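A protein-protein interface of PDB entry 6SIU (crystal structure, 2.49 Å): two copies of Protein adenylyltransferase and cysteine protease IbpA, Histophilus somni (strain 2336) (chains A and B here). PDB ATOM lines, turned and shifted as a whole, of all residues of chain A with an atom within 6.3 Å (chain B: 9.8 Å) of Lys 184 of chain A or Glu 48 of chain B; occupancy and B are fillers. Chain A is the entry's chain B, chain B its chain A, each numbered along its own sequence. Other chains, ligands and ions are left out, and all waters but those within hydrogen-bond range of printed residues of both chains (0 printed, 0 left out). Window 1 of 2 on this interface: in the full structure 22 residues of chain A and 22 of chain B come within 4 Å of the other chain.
The side-chain carboxylate (OD2) of Asp 44 of chain B sits at hydrogen-bond distance from the backbone NH (N) of Tyr 182 of chain A (2.7 Å).
The side-chain carboxylate of Glu 40 of chain B is in salt-bridge range of the guanidinium group of Arg 47 of chain B (3.3 Å).
The side-chain carboxylate (OD1) of Asp 44 of chain B is in salt-bridge range of the guanidinium group (NH1) of Arg 47 of chain B (2.6 Å).
NE of Arg 47 of chain B is in salt-bridge range of OD1 of Asp 69 of chain B, at 2.4 Å.
Among the printed residues, merely in contact across the chains: Leu 180 of chain A with Asp 44 of chain B, Leu 180 of chain A with Arg 47 of chain B, Tyr 182 of chain A with Lys 41 of chain B, Leu 180 of chain A with Glu 48 of chain B and Lys 184 of chain A with Glu 48 of chain B.
No residue of chain B comes within 4 Å of Glu 185 of chain A.
Printed residues of chain A within 4 Å of Lys 41 of chain B: Tyr 182 (3.8 Å).
Printed residues of chain A within 4 Å of Arg 47 of chain B: Leu 180 (3.7 Å).
Glu 48 of chain B touches just these residues of chain A: Leu 180 (3.8 Å) and Lys 184 (3.9 Å).
Ile 54 of chain B touches none of the printed residues of chain A.
Ile 71 of chain B touches none of the printed residues of chain A.
The nearest residue of chain A that does not touch Glu 48 of chain B is Lys 52 of chain A (5.7 Å).
Hydrophobic or aromatic side chains of chain A that line the printed part of chain B: Leu 180 and Tyr 182.
Printed residues of chain B that touch a printed residue of chain A: Lys 41, Asp 44, Arg 47 and Glu 48.
Among the printed residues, 6 pairs touch across the chains.
Positions printed for both chains: 45, 49, 52 and 184.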
ATOM      1  N   GLU A  45       7.629  -4.064 -12.433  1.00  0.00           N
ATOM      2  CA  GLU A  45       7.693  -4.406 -11.016  1.00  0.00           C
ATOM      3  C   GLU A  45       9.134  -4.418 -10.528  1.00  0.00           C
ATOM      4  O   GLU A  45       9.463  -3.812  -9.502  1.00  0.00           O
ATOM      5  CB  GLU A  45       7.028  -5.762 -10.785  1.00  0.00           C
ATOM      6  CG  GLU A  45       6.857  -6.159  -9.337  1.00  0.00           C
ATOM      7  CD  GLU A  45       6.241  -7.539  -9.217  1.00  0.00           C
ATOM      8  OE1 GLU A  45       6.849  -8.505  -9.732  1.00  0.00           O
ATOM      9  OE2 GLU A  45       5.139  -7.653  -8.638  1.00  0.00           O
ATOM     10  N   ILE A  49      10.764  -1.738  -7.709  1.00  0.00           N
ATOM     11  CA  ILE A  49      11.307  -2.273  -6.464  1.00  0.00           C
ATOM     12  C   ILE A  49      12.797  -1.963  -6.354  1.00  0.00           C
ATOM     13  O   ILE A  49      13.288  -1.578  -5.285  1.00  0.00           O
ATOM     14  CB  ILE A  49      11.022  -3.787  -6.365  1.00  0.00           C
ATOM     15  CG1 ILE A  49       9.521  -4.029  -6.214  1.00  0.00           C
ATOM     16  CG2 ILE A  49      11.740  -4.389  -5.191  1.00  0.00           C
ATOM     17  CD1 ILE A  49       9.148  -5.492  -6.066  1.00  0.00           C
ATOM     18  N   LYS A  52      13.707   1.695  -5.380  1.00  0.00           N
ATOM     19  CA  LYS A  52      13.402   2.132  -4.022  1.00  0.00           C
ATOM     20  C   LYS A  52      14.628   2.128  -3.124  1.00  0.00           C
ATOM     21  O   LYS A  52      14.673   2.889  -2.157  1.00  0.00           O
ATOM     22  CB  LYS A  52      12.303   1.248  -3.419  1.00  0.00           C
ATOM     23  CG  LYS A  52      10.904   1.495  -3.993  1.00  0.00           C
ATOM     24  CD  LYS A  52       9.820   0.780  -3.196  1.00  0.00           C
ATOM     25  CE  LYS A  52       8.428   1.163  -3.688  1.00  0.00           C
ATOM     26  NZ  LYS A  52       7.356   0.516  -2.883  1.00  0.00           N
ATOM     27  N   LEU A 180      -4.597  -7.961   1.607  1.00  0.00           N
ATOM     28  CA  LEU A 180      -4.340  -8.195   0.195  1.00  0.00           C
ATOM     29  C   LEU A 180      -4.400  -9.682  -0.103  1.00  0.00           C
ATOM     30  O   LEU A 180      -3.885 -10.502   0.657  1.00  0.00           O
ATOM     31  CB  LEU A 180      -2.972  -7.644  -0.208  1.00  0.00           C
ATOM     32  CG  LEU A 180      -2.875  -6.180  -0.624  1.00  0.00           C
ATOM     33  CD1 LEU A 180      -3.242  -5.287   0.530  1.00  0.00           C
ATOM     34  CD2 LEU A 180      -1.474  -5.880  -1.120  1.00  0.00           C
ATOM     35  N   TYR A 182      -3.085 -11.216  -3.064  1.00  0.00           N
ATOM     36  CA  TYR A 182      -1.760 -11.561  -3.538  1.00  0.00           C
ATOM     37  C   TYR A 182      -0.699 -10.868  -2.692  1.00  0.00           C
ATOM     38  O   TYR A 182      -0.948  -9.846  -2.045  1.00  0.00           O
ATOM     39  CB  TYR A 182      -1.605 -11.177  -5.009  1.00  0.00           C
ATOM     40  CG  TYR A 182      -2.451 -12.005  -5.951  1.00  0.00           C
ATOM     41  CD1 TYR A 182      -2.006 -13.239  -6.405  1.00  0.00           C
ATOM     42  CD2 TYR A 182      -3.689 -11.552  -6.388  1.00  0.00           C
ATOM     43  CE1 TYR A 182      -2.770 -13.998  -7.269  1.00  0.00           C
ATOM     44  CE2 TYR A 182      -4.464 -12.307  -7.251  1.00  0.00           C
ATOM     45  CZ  TYR A 182      -3.998 -13.527  -7.691  1.00  0.00           C
ATOM     46  OH  TYR A 182      -4.766 -14.277  -8.554  1.00  0.00           O
ATOM     47  N   LYS A 183       0.497 -11.445  -2.691  1.00  0.00           N
ATOM     48  CA  LYS A 183       1.599 -10.806  -1.994  1.00  0.00           C
ATOM     49  C   LYS A 183       1.970  -9.507  -2.694  1.00  0.00           C
ATOM     50  O   LYS A 183       1.764  -9.344  -3.899  1.00  0.00           O
ATOM     51  CB  LYS A 183       2.806 -11.739  -1.920  1.00  0.00           C
ATOM     52  CG  LYS A 183       3.338 -12.163  -3.271  1.00  0.00           C
ATOM     53  CD  LYS A 183       4.485 -13.148  -3.124  1.00  0.00           C
ATOM     54  CE  LYS A 183       5.062 -13.509  -4.480  1.00  0.00           C
ATOM     55  NZ  LYS A 183       6.099 -14.573  -4.363  1.00  0.00           N
ATOM     56  N   LYS A 184       2.498  -8.567  -1.918  1.00  0.00           N
ATOM     57  CA  LYS A 184       2.876  -7.257  -2.427  1.00  0.00           C
ATOM     58  C   LYS A 184       4.374  -7.122  -2.644  1.00  0.00           C
ATOM     59  O   LYS A 184       4.826  -6.082  -3.129  1.00  0.00           O
ATOM     60  CB  LYS A 184       2.381  -6.157  -1.474  1.00  0.00           C
ATOM     61  CG  LYS A 184       2.984  -6.234  -0.082  1.00  0.00           C
ATOM     62  CD  LYS A 184       2.402  -5.198   0.878  1.00  0.00           C
ATOM     63  CE  LYS A 184       2.965  -5.400   2.284  1.00  0.00           C
ATOM     64  NZ  LYS A 184       2.432  -4.422   3.279  1.00  0.00           N
ATOM     65  N   GLU A 185       5.152  -8.144  -2.303  1.00  0.00           N
ATOM     66  CA  GLU A 185       6.601  -8.074  -2.433  1.00  0.00           C
ATOM     67  C   GLU A 185       7.156  -9.485  -2.494  1.00  0.00           C
ATOM     68  O   GLU A 185       6.473 -10.457  -2.165  1.00  0.00           O
ATOM     69  CB  GLU A 185       7.236  -7.311  -1.268  1.00  0.00           C
ATOM     70  CG  GLU A 185       6.972  -7.961   0.077  1.00  0.00           C
ATOM     71  CD  GLU A 185       7.297  -7.054   1.247  1.00  0.00           C
ATOM     72  OE1 GLU A 185       8.213  -6.212   1.113  1.00  0.00           O
ATOM     73  OE2 GLU A 185       6.630  -7.180   2.297  1.00  0.00           O
ATOM     74  N   ASN A 186       8.408  -9.581  -2.925  1.00  0.00           N
ATOM     75  CA  ASN A 186       9.098 -10.860  -2.897  1.00  0.00           C
ATOM     76  C   ASN A 186       9.328 -11.293  -1.456  1.00  0.00           C
ATOM     77  O   ASN A 186       9.845 -10.525  -0.633  1.00  0.00           O
ATOM     78  CB  ASN A 186      10.417 -10.772  -3.645  1.00  0.00           C
ATOM     79  CG  ASN A 186      10.238 -10.930  -5.120  1.00  0.00           C
ATOM     80  OD1 ASN A 186       9.832  -9.994  -5.806  1.00  0.00           O
ATOM     81  ND2 ASN A 186      10.519 -12.122  -5.626  1.00  0.00           N
ATOM     82  N   PRO A 197       5.830 -11.130  -7.157  1.00  0.00           N
ATOM     83  CA  PRO A 197       4.359 -11.101  -7.200  1.00  0.00           C
ATOM     84  C   PRO A 197       3.807 -11.173  -8.611  1.00  0.00           C
ATOM     85  O   PRO A 197       2.891 -11.961  -8.867  1.00  0.00           O
ATOM     86  CB  PRO A 197       4.028  -9.769  -6.517  1.00  0.00           C
ATOM     87  CG  PRO A 197       5.189  -9.518  -5.605  1.00  0.00           C
ATOM     88  CD  PRO A 197       6.388 -10.043  -6.331  1.00  0.00           C
ATOM     89  N   ALA A 239      -0.581 -13.931  -0.552  1.00  0.00           N
ATOM     90  CA  ALA A 239       0.036 -13.381   0.646  1.00  0.00           C
ATOM     91  C   ALA A 239       0.123 -14.434   1.740  1.00  0.00           C
ATOM     92  O   ALA A 239       1.105 -14.487   2.491  1.00  0.00           O
ATOM     93  CB  ALA A 239      -0.756 -12.170   1.130  1.00  0.00           C
ATOM     94  N   GLU B  40      -9.262  -9.169  -8.749  1.00  0.00           N
ATOM     95  CA  GLU B  40      -8.515  -9.094  -7.497  1.00  0.00           C
ATOM     96  C   GLU B  40      -7.202  -8.337  -7.651  1.00  0.00           C
ATOM     97  O   GLU B  40      -6.763  -7.675  -6.703  1.00  0.00           O
ATOM     98  CB  GLU B  40      -8.255 -10.494  -6.953  1.00  0.00           C
ATOM     99  CG  GLU B  40      -9.514 -11.194  -6.499  1.00  0.00           C
ATOM    100  CD  GLU B  40     -10.160 -10.512  -5.306  1.00  0.00           C
ATOM    101  OE1 GLU B  40      -9.424  -9.934  -4.477  1.00  0.00           O
ATOM    102  OE2 GLU B  40     -11.404 -10.552  -5.200  1.00  0.00           O
ATOM    103  N   LYS B  41      -6.555  -8.422  -8.817  1.00  0.00           N
ATOM    104  CA  LYS B  41      -5.382  -7.586  -9.055  1.00  0.00           C
ATOM    105  C   LYS B  41      -5.747  -6.113  -8.961  1.00  0.00           C
ATOM    106  O   LYS B  41      -4.977  -5.306  -8.429  1.00  0.00           O
ATOM    107  CB  LYS B  41      -4.765  -7.898 -10.417  1.00  0.00           C
ATOM    108  CG  LYS B  41      -3.928  -9.177 -10.473  1.00  0.00           C
ATOM    109  CD  LYS B  41      -4.784 -10.443 -10.560  1.00  0.00           C
ATOM    110  CE  LYS B  41      -5.412 -10.624 -11.941  1.00  0.00           C
ATOM    111  NZ  LYS B  41      -6.269 -11.850 -12.019  1.00  0.00           N
ATOM    112  N   PHE B  42      -6.928  -5.746  -9.459  1.00  0.00           N
ATOM    113  CA  PHE B  42      -7.382  -4.366  -9.330  1.00  0.00           C
ATOM    114  C   PHE B  42      -7.704  -4.029  -7.881  1.00  0.00           C
ATOM    115  O   PHE B  42      -7.315  -2.969  -7.382  1.00  0.00           O
ATOM    116  CB  PHE B  42      -8.597  -4.125 -10.222  1.00  0.00           C
ATOM    117  CG  PHE B  42      -9.312  -2.831  -9.943  1.00  0.00           C
ATOM    118  CD1 PHE B  42      -8.843  -1.634 -10.461  1.00  0.00           C
ATOM    119  CD2 PHE B  42     -10.462  -2.815  -9.174  1.00  0.00           C
ATOM    120  CE1 PHE B  42      -9.507  -0.446 -10.211  1.00  0.00           C
ATOM    121  CE2 PHE B  42     -11.129  -1.628  -8.917  1.00  0.00           C
ATOM    122  CZ  PHE B  42     -10.652  -0.444  -9.437  1.00  0.00           C
ATOM    123  N   LEU B  43      -8.417  -4.914  -7.187  1.00  0.00           N
ATOM    124  CA  LEU B  43      -8.769  -4.617  -5.803  1.00  0.00           C
ATOM    125  C   LEU B  43      -7.533  -4.588  -4.918  1.00  0.00           C
ATOM    126  O   LEU B  43      -7.416  -3.724  -4.041  1.00  0.00           O
ATOM    127  CB  LEU B  43      -9.775  -5.637  -5.284  1.00  0.00           C
ATOM    128  CG  LEU B  43     -11.095  -5.642  -6.045  1.00  0.00           C
ATOM    129  CD1 LEU B  43     -11.891  -6.861  -5.680  1.00  0.00           C
ATOM    130  CD2 LEU B  43     -11.866  -4.376  -5.746  1.00  0.00           C
ATOM    131  N   ASP B  44      -6.596  -5.515  -5.142  1.00  0.00           N
ATOM    132  CA  ASP B  44      -5.367  -5.517  -4.354  1.00  0.00           C
ATOM    133  C   ASP B  44      -4.617  -4.198  -4.504  1.00  0.00           C
ATOM    134  O   ASP B  44      -4.092  -3.660  -3.521  1.00  0.00           O
ATOM    135  CB  ASP B  44      -4.482  -6.701  -4.755  1.00  0.00           C
ATOM    136  CG  ASP B  44      -4.743  -7.953  -3.915  1.00  0.00           C
ATOM    137  OD1 ASP B  44      -5.641  -7.929  -3.047  1.00  0.00           O
ATOM    138  OD2 ASP B  44      -4.038  -8.966  -4.123  1.00  0.00           O
ATOM    139  N   GLU B  45      -4.583  -3.646  -5.719  1.00  0.00           N
ATOM    140  CA  GLU B  45      -3.930  -2.355  -5.929  1.00  0.00           C
ATOM    141  C   GLU B  45      -4.603  -1.262  -5.106  1.00  0.00           C
ATOM    142  O   GLU B  45      -3.927  -0.466  -4.443  1.00  0.00           O
ATOM    143  CB  GLU B  45      -3.932  -2.001  -7.415  1.00  0.00           C
ATOM    144  CG  GLU B  45      -3.099  -0.796  -7.779  1.00  0.00           C
ATOM    145  CD  GLU B  45      -3.177  -0.466  -9.260  1.00  0.00           C
ATOM    146  OE1 GLU B  45      -4.299  -0.205  -9.755  1.00  0.00           O
ATOM    147  OE2 GLU B  45      -2.121  -0.475  -9.928  1.00  0.00           O
ATOM    148  N   ALA B  46      -5.938  -1.220  -5.121  1.00  0.00           N
ATOM    149  CA  ALA B  46      -6.662  -0.247  -4.310  1.00  0.00           C
ATOM    150  C   ALA B  46      -6.421  -0.474  -2.826  1.00  0.00           C
ATOM    151  O   ALA B  46      -6.268   0.487  -2.064  1.00  0.00           O
ATOM    152  CB  ALA B  46      -8.154  -0.311  -4.618  1.00  0.00           C
ATOM    153  N   ARG B  47      -6.390  -1.736  -2.397  1.00  0.00           N
ATOM    154  CA  ARG B  47      -6.148  -2.031  -0.988  1.00  0.00           C
ATOM    155  C   ARG B  47      -4.784  -1.514  -0.545  1.00  0.00           C
ATOM    156  O   ARG B  47      -4.664  -0.865   0.500  1.00  0.00           O
ATOM    157  CB  ARG B  47      -6.255  -3.535  -0.731  1.00  0.00           C
ATOM    158  CG  ARG B  47      -7.649  -4.109  -0.863  1.00  0.00           C
ATOM    159  CD  ARG B  47      -7.608  -5.621  -0.687  1.00  0.00           C
ATOM    160  NE  ARG B  47      -8.896  -6.247  -0.959  1.00  0.00           N
ATOM    161  CZ  ARG B  47      -9.132  -7.053  -1.989  1.00  0.00           C
ATOM    162  NH1 ARG B  47      -8.162  -7.346  -2.838  1.00  0.00           N
ATOM    163  NH2 ARG B  47     -10.337  -7.578  -2.156  1.00  0.00           N
ATOM    164  N   GLU B  48      -3.738  -1.792  -1.332  1.00  0.00           N
ATOM    165  CA  GLU B  48      -2.395  -1.414  -0.904  1.00  0.00           C
ATOM    166  C   GLU B  48      -2.221   0.099  -0.910  1.00  0.00           C
ATOM    167  O   GLU B  48      -1.656   0.665   0.033  1.00  0.00           O
ATOM    168  CB  GLU B  48      -1.338  -2.090  -1.783  1.00  0.00           C
ATOM    169  CG  GLU B  48       0.107  -1.754  -1.398  1.00  0.00           C
ATOM    170  CD  GLU B  48       1.143  -2.334  -2.361  1.00  0.00           C
ATOM    171  OE1 GLU B  48       0.753  -3.100  -3.271  1.00  0.00           O
ATOM    172  OE2 GLU B  48       2.346  -2.023  -2.210  1.00  0.00           O
ATOM    173  N   ILE B  49      -2.706   0.772  -1.955  1.00  0.00           N
ATOM    174  CA  ILE B  49      -2.591   2.227  -2.010  1.00  0.00           C
ATOM    175  C   ILE B  49      -3.355   2.863  -0.856  1.00  0.00           C
ATOM    176  O   ILE B  49      -2.840   3.751  -0.165  1.00  0.00           O
ATOM    177  CB  ILE B  49      -3.076   2.759  -3.373  1.00  0.00           C
ATOM    178  CG1 ILE B  49      -2.158   2.273  -4.498  1.00  0.00           C
ATOM    179  CG2 ILE B  49      -3.125   4.275  -3.363  1.00  0.00           C
ATOM    180  CD1 ILE B  49      -2.558   2.765  -5.884  1.00  0.00           C
ATOM    181  N   SER B  50      -4.588   2.413  -0.619  1.00  0.00           N
ATOM    182  CA  SER B  50      -5.394   2.992   0.452  1.00  0.00           C
ATOM    183  C   SER B  50      -4.723   2.814   1.806  1.00  0.00           C
ATOM    184  O   SER B  50      -4.692   3.742   2.621  1.00  0.00           O
ATOM    185  CB  SER B  50      -6.791   2.368   0.460  1.00  0.00           C
ATOM    186  OG  SER B  50      -7.458   2.641  -0.760  1.00  0.00           O
ATOM    187  N   LYS B  51      -4.173   1.630   2.066  1.00  0.00           N
ATOM    188  CA  LYS B  51      -3.555   1.382   3.360  1.00  0.00           C
ATOM    189  C   LYS B  51      -2.289   2.204   3.570  1.00  0.00           C
ATOM    190  O   LYS B  51      -1.919   2.450   4.724  1.00  0.00           O
ATOM    191  CB  LYS B  51      -3.246  -0.101   3.517  1.00  0.00           C
ATOM    192  CG  LYS B  51      -4.463  -0.971   3.749  1.00  0.00           C
ATOM    193  CD  LYS B  51      -4.055  -2.432   3.825  1.00  0.00           C
ATOM    194  CE  LYS B  51      -5.008  -3.234   4.673  1.00  0.00           C
ATOM    195  NZ  LYS B  51      -4.537  -4.639   4.833  1.00  0.00           N
ATOM    196  N   LYS B  52      -1.619   2.640   2.494  1.00  0.00           N
ATOM    197  CA  LYS B  52      -0.403   3.435   2.660  1.00  0.00           C
ATOM    198  C   LYS B  52      -0.670   4.713   3.444  1.00  0.00           C
ATOM    199  O   LYS B  52       0.231   5.238   4.106  1.00  0.00           O
ATOM    200  CB  LYS B  52       0.204   3.784   1.299  1.00  0.00           C
ATOM    201  CG  LYS B  52       0.915   2.637   0.604  1.00  0.00           C
ATOM    202  CD  LYS B  52       1.484   3.080  -0.745  1.00  0.00           C
ATOM    203  CE  LYS B  52       2.276   1.970  -1.416  1.00  0.00           C
ATOM    204  NZ  LYS B  52       3.438   1.525  -0.592  1.00  0.00           N
ATOM    205  N   SER B  53      -1.893   5.222   3.383  1.00  0.00           N
ATOM    206  CA  SER B  53      -2.248   6.465   4.039  1.00  0.00           C
ATOM    207  C   SER B  53      -2.890   6.250   5.402  1.00  0.00           C
ATOM    208  O   SER B  53      -3.171   7.228   6.096  1.00  0.00           O
ATOM    209  CB  SER B  53      -3.181   7.274   3.134  1.00  0.00           C
ATOM    210  OG  SER B  53      -3.572   8.479   3.759  1.00  0.00           O
ATOM    211  N   ILE B  54      -3.116   5.008   5.805  1.00  0.00           N
ATOM    212  CA  ILE B  54      -3.823   4.693   7.044  1.00  0.00           C
ATOM    213  C   ILE B  54      -2.803   4.257   8.093  1.00  0.00           C
ATOM    214  O   ILE B  54      -1.986   3.373   7.808  1.00  0.00           O
ATOM    215  CB  ILE B  54      -4.882   3.597   6.832  1.00  0.00           C
ATOM    216  CG1 ILE B  54      -5.826   3.968   5.690  1.00  0.00           C
ATOM    217  CG2 ILE B  54      -5.689   3.402   8.093  1.00  0.00           C
ATOM    218  CD1 ILE B  54      -6.907   2.931   5.449  1.00  0.00           C
ATOM    219  N   GLU B  56      -0.965   2.282  11.046  1.00  0.00           N
ATOM    220  CA  GLU B  56      -0.990   0.850  11.316  1.00  0.00           C
ATOM    221  C   GLU B  56      -1.946   0.516  12.450  1.00  0.00           C
ATOM    222  O   GLU B  56      -2.585  -0.543  12.433  1.00  0.00           O
ATOM    223  CB  GLU B  56       0.419   0.350  11.640  1.00  0.00           C
ATOM    224  CG  GLU B  56       0.552  -1.165  11.707  1.00  0.00           C
ATOM    225  CD  GLU B  56       1.982  -1.620  11.960  1.00  0.00           C
ATOM    226  OE1 GLU B  56       2.814  -0.781  12.368  1.00  0.00           O
ATOM    227  OE2 GLU B  56       2.275  -2.817  11.747  1.00  0.00           O
ATOM    228  N   VAL B  59      -5.395   0.366  10.931  1.00  0.00           N
ATOM    229  CA  VAL B  59      -5.611  -0.823  10.111  1.00  0.00           C
ATOM    230  C   VAL B  59      -5.955  -2.017  10.987  1.00  0.00           C
ATOM    231  O   VAL B  59      -6.858  -2.801  10.670  1.00  0.00           O
ATOM    232  CB  VAL B  59      -4.378  -1.108   9.238  1.00  0.00           C
ATOM    233  CG1 VAL B  59      -4.554  -2.427   8.503  1.00  0.00           C
ATOM    234  CG2 VAL B  59      -4.143   0.033   8.260  1.00  0.00           C
ATOM    235  N   PHE B  68     -14.417  -3.076   6.089  1.00  0.00           N
ATOM    236  CA  PHE B  68     -13.128  -2.442   5.843  1.00  0.00           C
ATOM    237  C   PHE B  68     -12.686  -2.626   4.395  1.00  0.00           C
ATOM    238  O   PHE B  68     -12.241  -1.666   3.752  1.00  0.00           O
ATOM    239  CB  PHE B  68     -12.080  -3.011   6.799  1.00  0.00           C
ATOM    240  CG  PHE B  68     -10.739  -2.327   6.714  1.00  0.00           C
ATOM    241  CD1 PHE B  68     -10.639  -0.991   6.358  1.00  0.00           C
ATOM    242  CD2 PHE B  68      -9.573  -3.029   6.991  1.00  0.00           C
ATOM    243  CE1 PHE B  68      -9.404  -0.367   6.285  1.00  0.00           C
ATOM    244  CE2 PHE B  68      -8.342  -2.413   6.921  1.00  0.00           C
ATOM    245  CZ  PHE B  68      -8.254  -1.082   6.563  1.00  0.00           C
ATOM    246  N   ASP B  69     -12.823  -3.840   3.853  1.00  0.00           N
ATOM    247  CA  ASP B  69     -12.332  -4.071   2.500  1.00  0.00           C
ATOM    248  C   ASP B  69     -13.092  -3.228   1.482  1.00  0.00           C
ATOM    249  O   ASP B  69     -12.498  -2.717   0.526  1.00  0.00           O
ATOM    250  CB  ASP B  69     -12.416  -5.550   2.151  1.00  0.00           C
ATOM    251  CG  ASP B  69     -11.679  -5.876   0.862  1.00  0.00           C
ATOM    252  OD1 ASP B  69     -10.456  -5.627   0.795  1.00  0.00           O
ATOM    253  OD2 ASP B  69     -12.329  -6.370  -0.084  1.00  0.00           O
ATOM    254  N   ILE B  71     -14.315  -0.291   2.079  1.00  0.00           N
ATOM    255  CA  ILE B  71     -13.861   1.087   2.234  1.00  0.00           C
ATOM    256  C   ILE B  71     -12.558   1.299   1.478  1.00  0.00           C
ATOM    257  O   ILE B  71     -12.337   2.358   0.878  1.00  0.00           O
ATOM    258  CB  ILE B  71     -13.725   1.433   3.728  1.00  0.00           C
ATOM    259  CG1 ILE B  71     -15.079   1.291   4.414  1.00  0.00           C
ATOM    260  CG2 ILE B  71     -13.217   2.845   3.917  1.00  0.00           C
ATOM    261  CD1 ILE B  71     -15.047   1.532   5.887  1.00  0.00           C
ATOM    262  N   LEU B  72     -11.684   0.290   1.472  1.00  0.00           N
ATOM    263  CA  LEU B  72     -10.412   0.415   0.772  1.00  0.00           C
ATOM    264  C   LEU B  72     -10.598   0.504  -0.739  1.00  0.00           C
ATOM    265  O   LEU B  72      -9.803   1.163  -1.420  1.00  0.00           O
ATOM    266  CB  LEU B  72      -9.503  -0.765   1.124  1.00  0.00           C
ATOM    267  CG  LEU B  72      -9.074  -0.908   2.590  1.00  0.00           C
ATOM    268  CD1 LEU B  72      -8.210  -2.147   2.771  1.00  0.00           C
ATOM    269  CD2 LEU B  72      -8.340   0.329   3.061  1.00  0.00           C
ATOM    270  N   THR B  73     -11.640  -0.129  -1.283  1.00  0.00           N
ATOM    271  CA  THR B  73     -11.806  -0.226  -2.727  1.00  0.00           C
ATOM    272  C   THR B  73     -12.966   0.587  -3.282  1.00  0.00           C
ATOM    273  O   THR B  73     -13.089   0.680  -4.507  1.00  0.00           O
ATOM    274  CB  THR B  73     -11.991  -1.691  -3.147  1.00  0.00           C
ATOM    275  OG1 THR B  73     -13.226  -2.187  -2.617  1.00  0.00           O
ATOM    276  CG2 THR B  73     -10.840  -2.543  -2.632  1.00  0.00           C
ATOM    277  N   ALA B  76     -11.786   3.626  -5.584  1.00  0.00           N
ATOM    278  CA  ALA B  76     -11.228   3.176  -6.856  1.00  0.00           C
ATOM    279  C   ALA B  76     -12.313   2.638  -7.779  1.00  0.00           C
ATOM    280  O   ALA B  76     -12.268   2.858  -8.996  1.00  0.00           O
ATOM    281  CB  ALA B  76     -10.168   2.105  -6.612  1.00  0.00           C
ATOM    282  N   LYS B 184       2.866   4.217 -12.327  1.00  0.00           N
ATOM    283  CA  LYS B 184       2.945   3.548 -11.038  1.00  0.00           C
ATOM    284  C   LYS B 184       1.865   3.995 -10.067  1.00  0.00           C
ATOM    285  O   LYS B 184       1.746   3.408  -8.989  1.00  0.00           O
ATOM    286  CB  LYS B 184       4.331   3.767 -10.409  1.00  0.00           C
ATOM    287  CG  LYS B 184       4.683   5.223 -10.160  1.00  0.00           C
ATOM    288  CD  LYS B 184       6.194   5.413  -9.979  1.00  0.00           C
ATOM    289  CE  LYS B 184       6.715   4.740  -8.721  1.00  0.00           C
ATOM    290  NZ  LYS B 184       6.320   5.467  -7.478  1.00  0.00           N
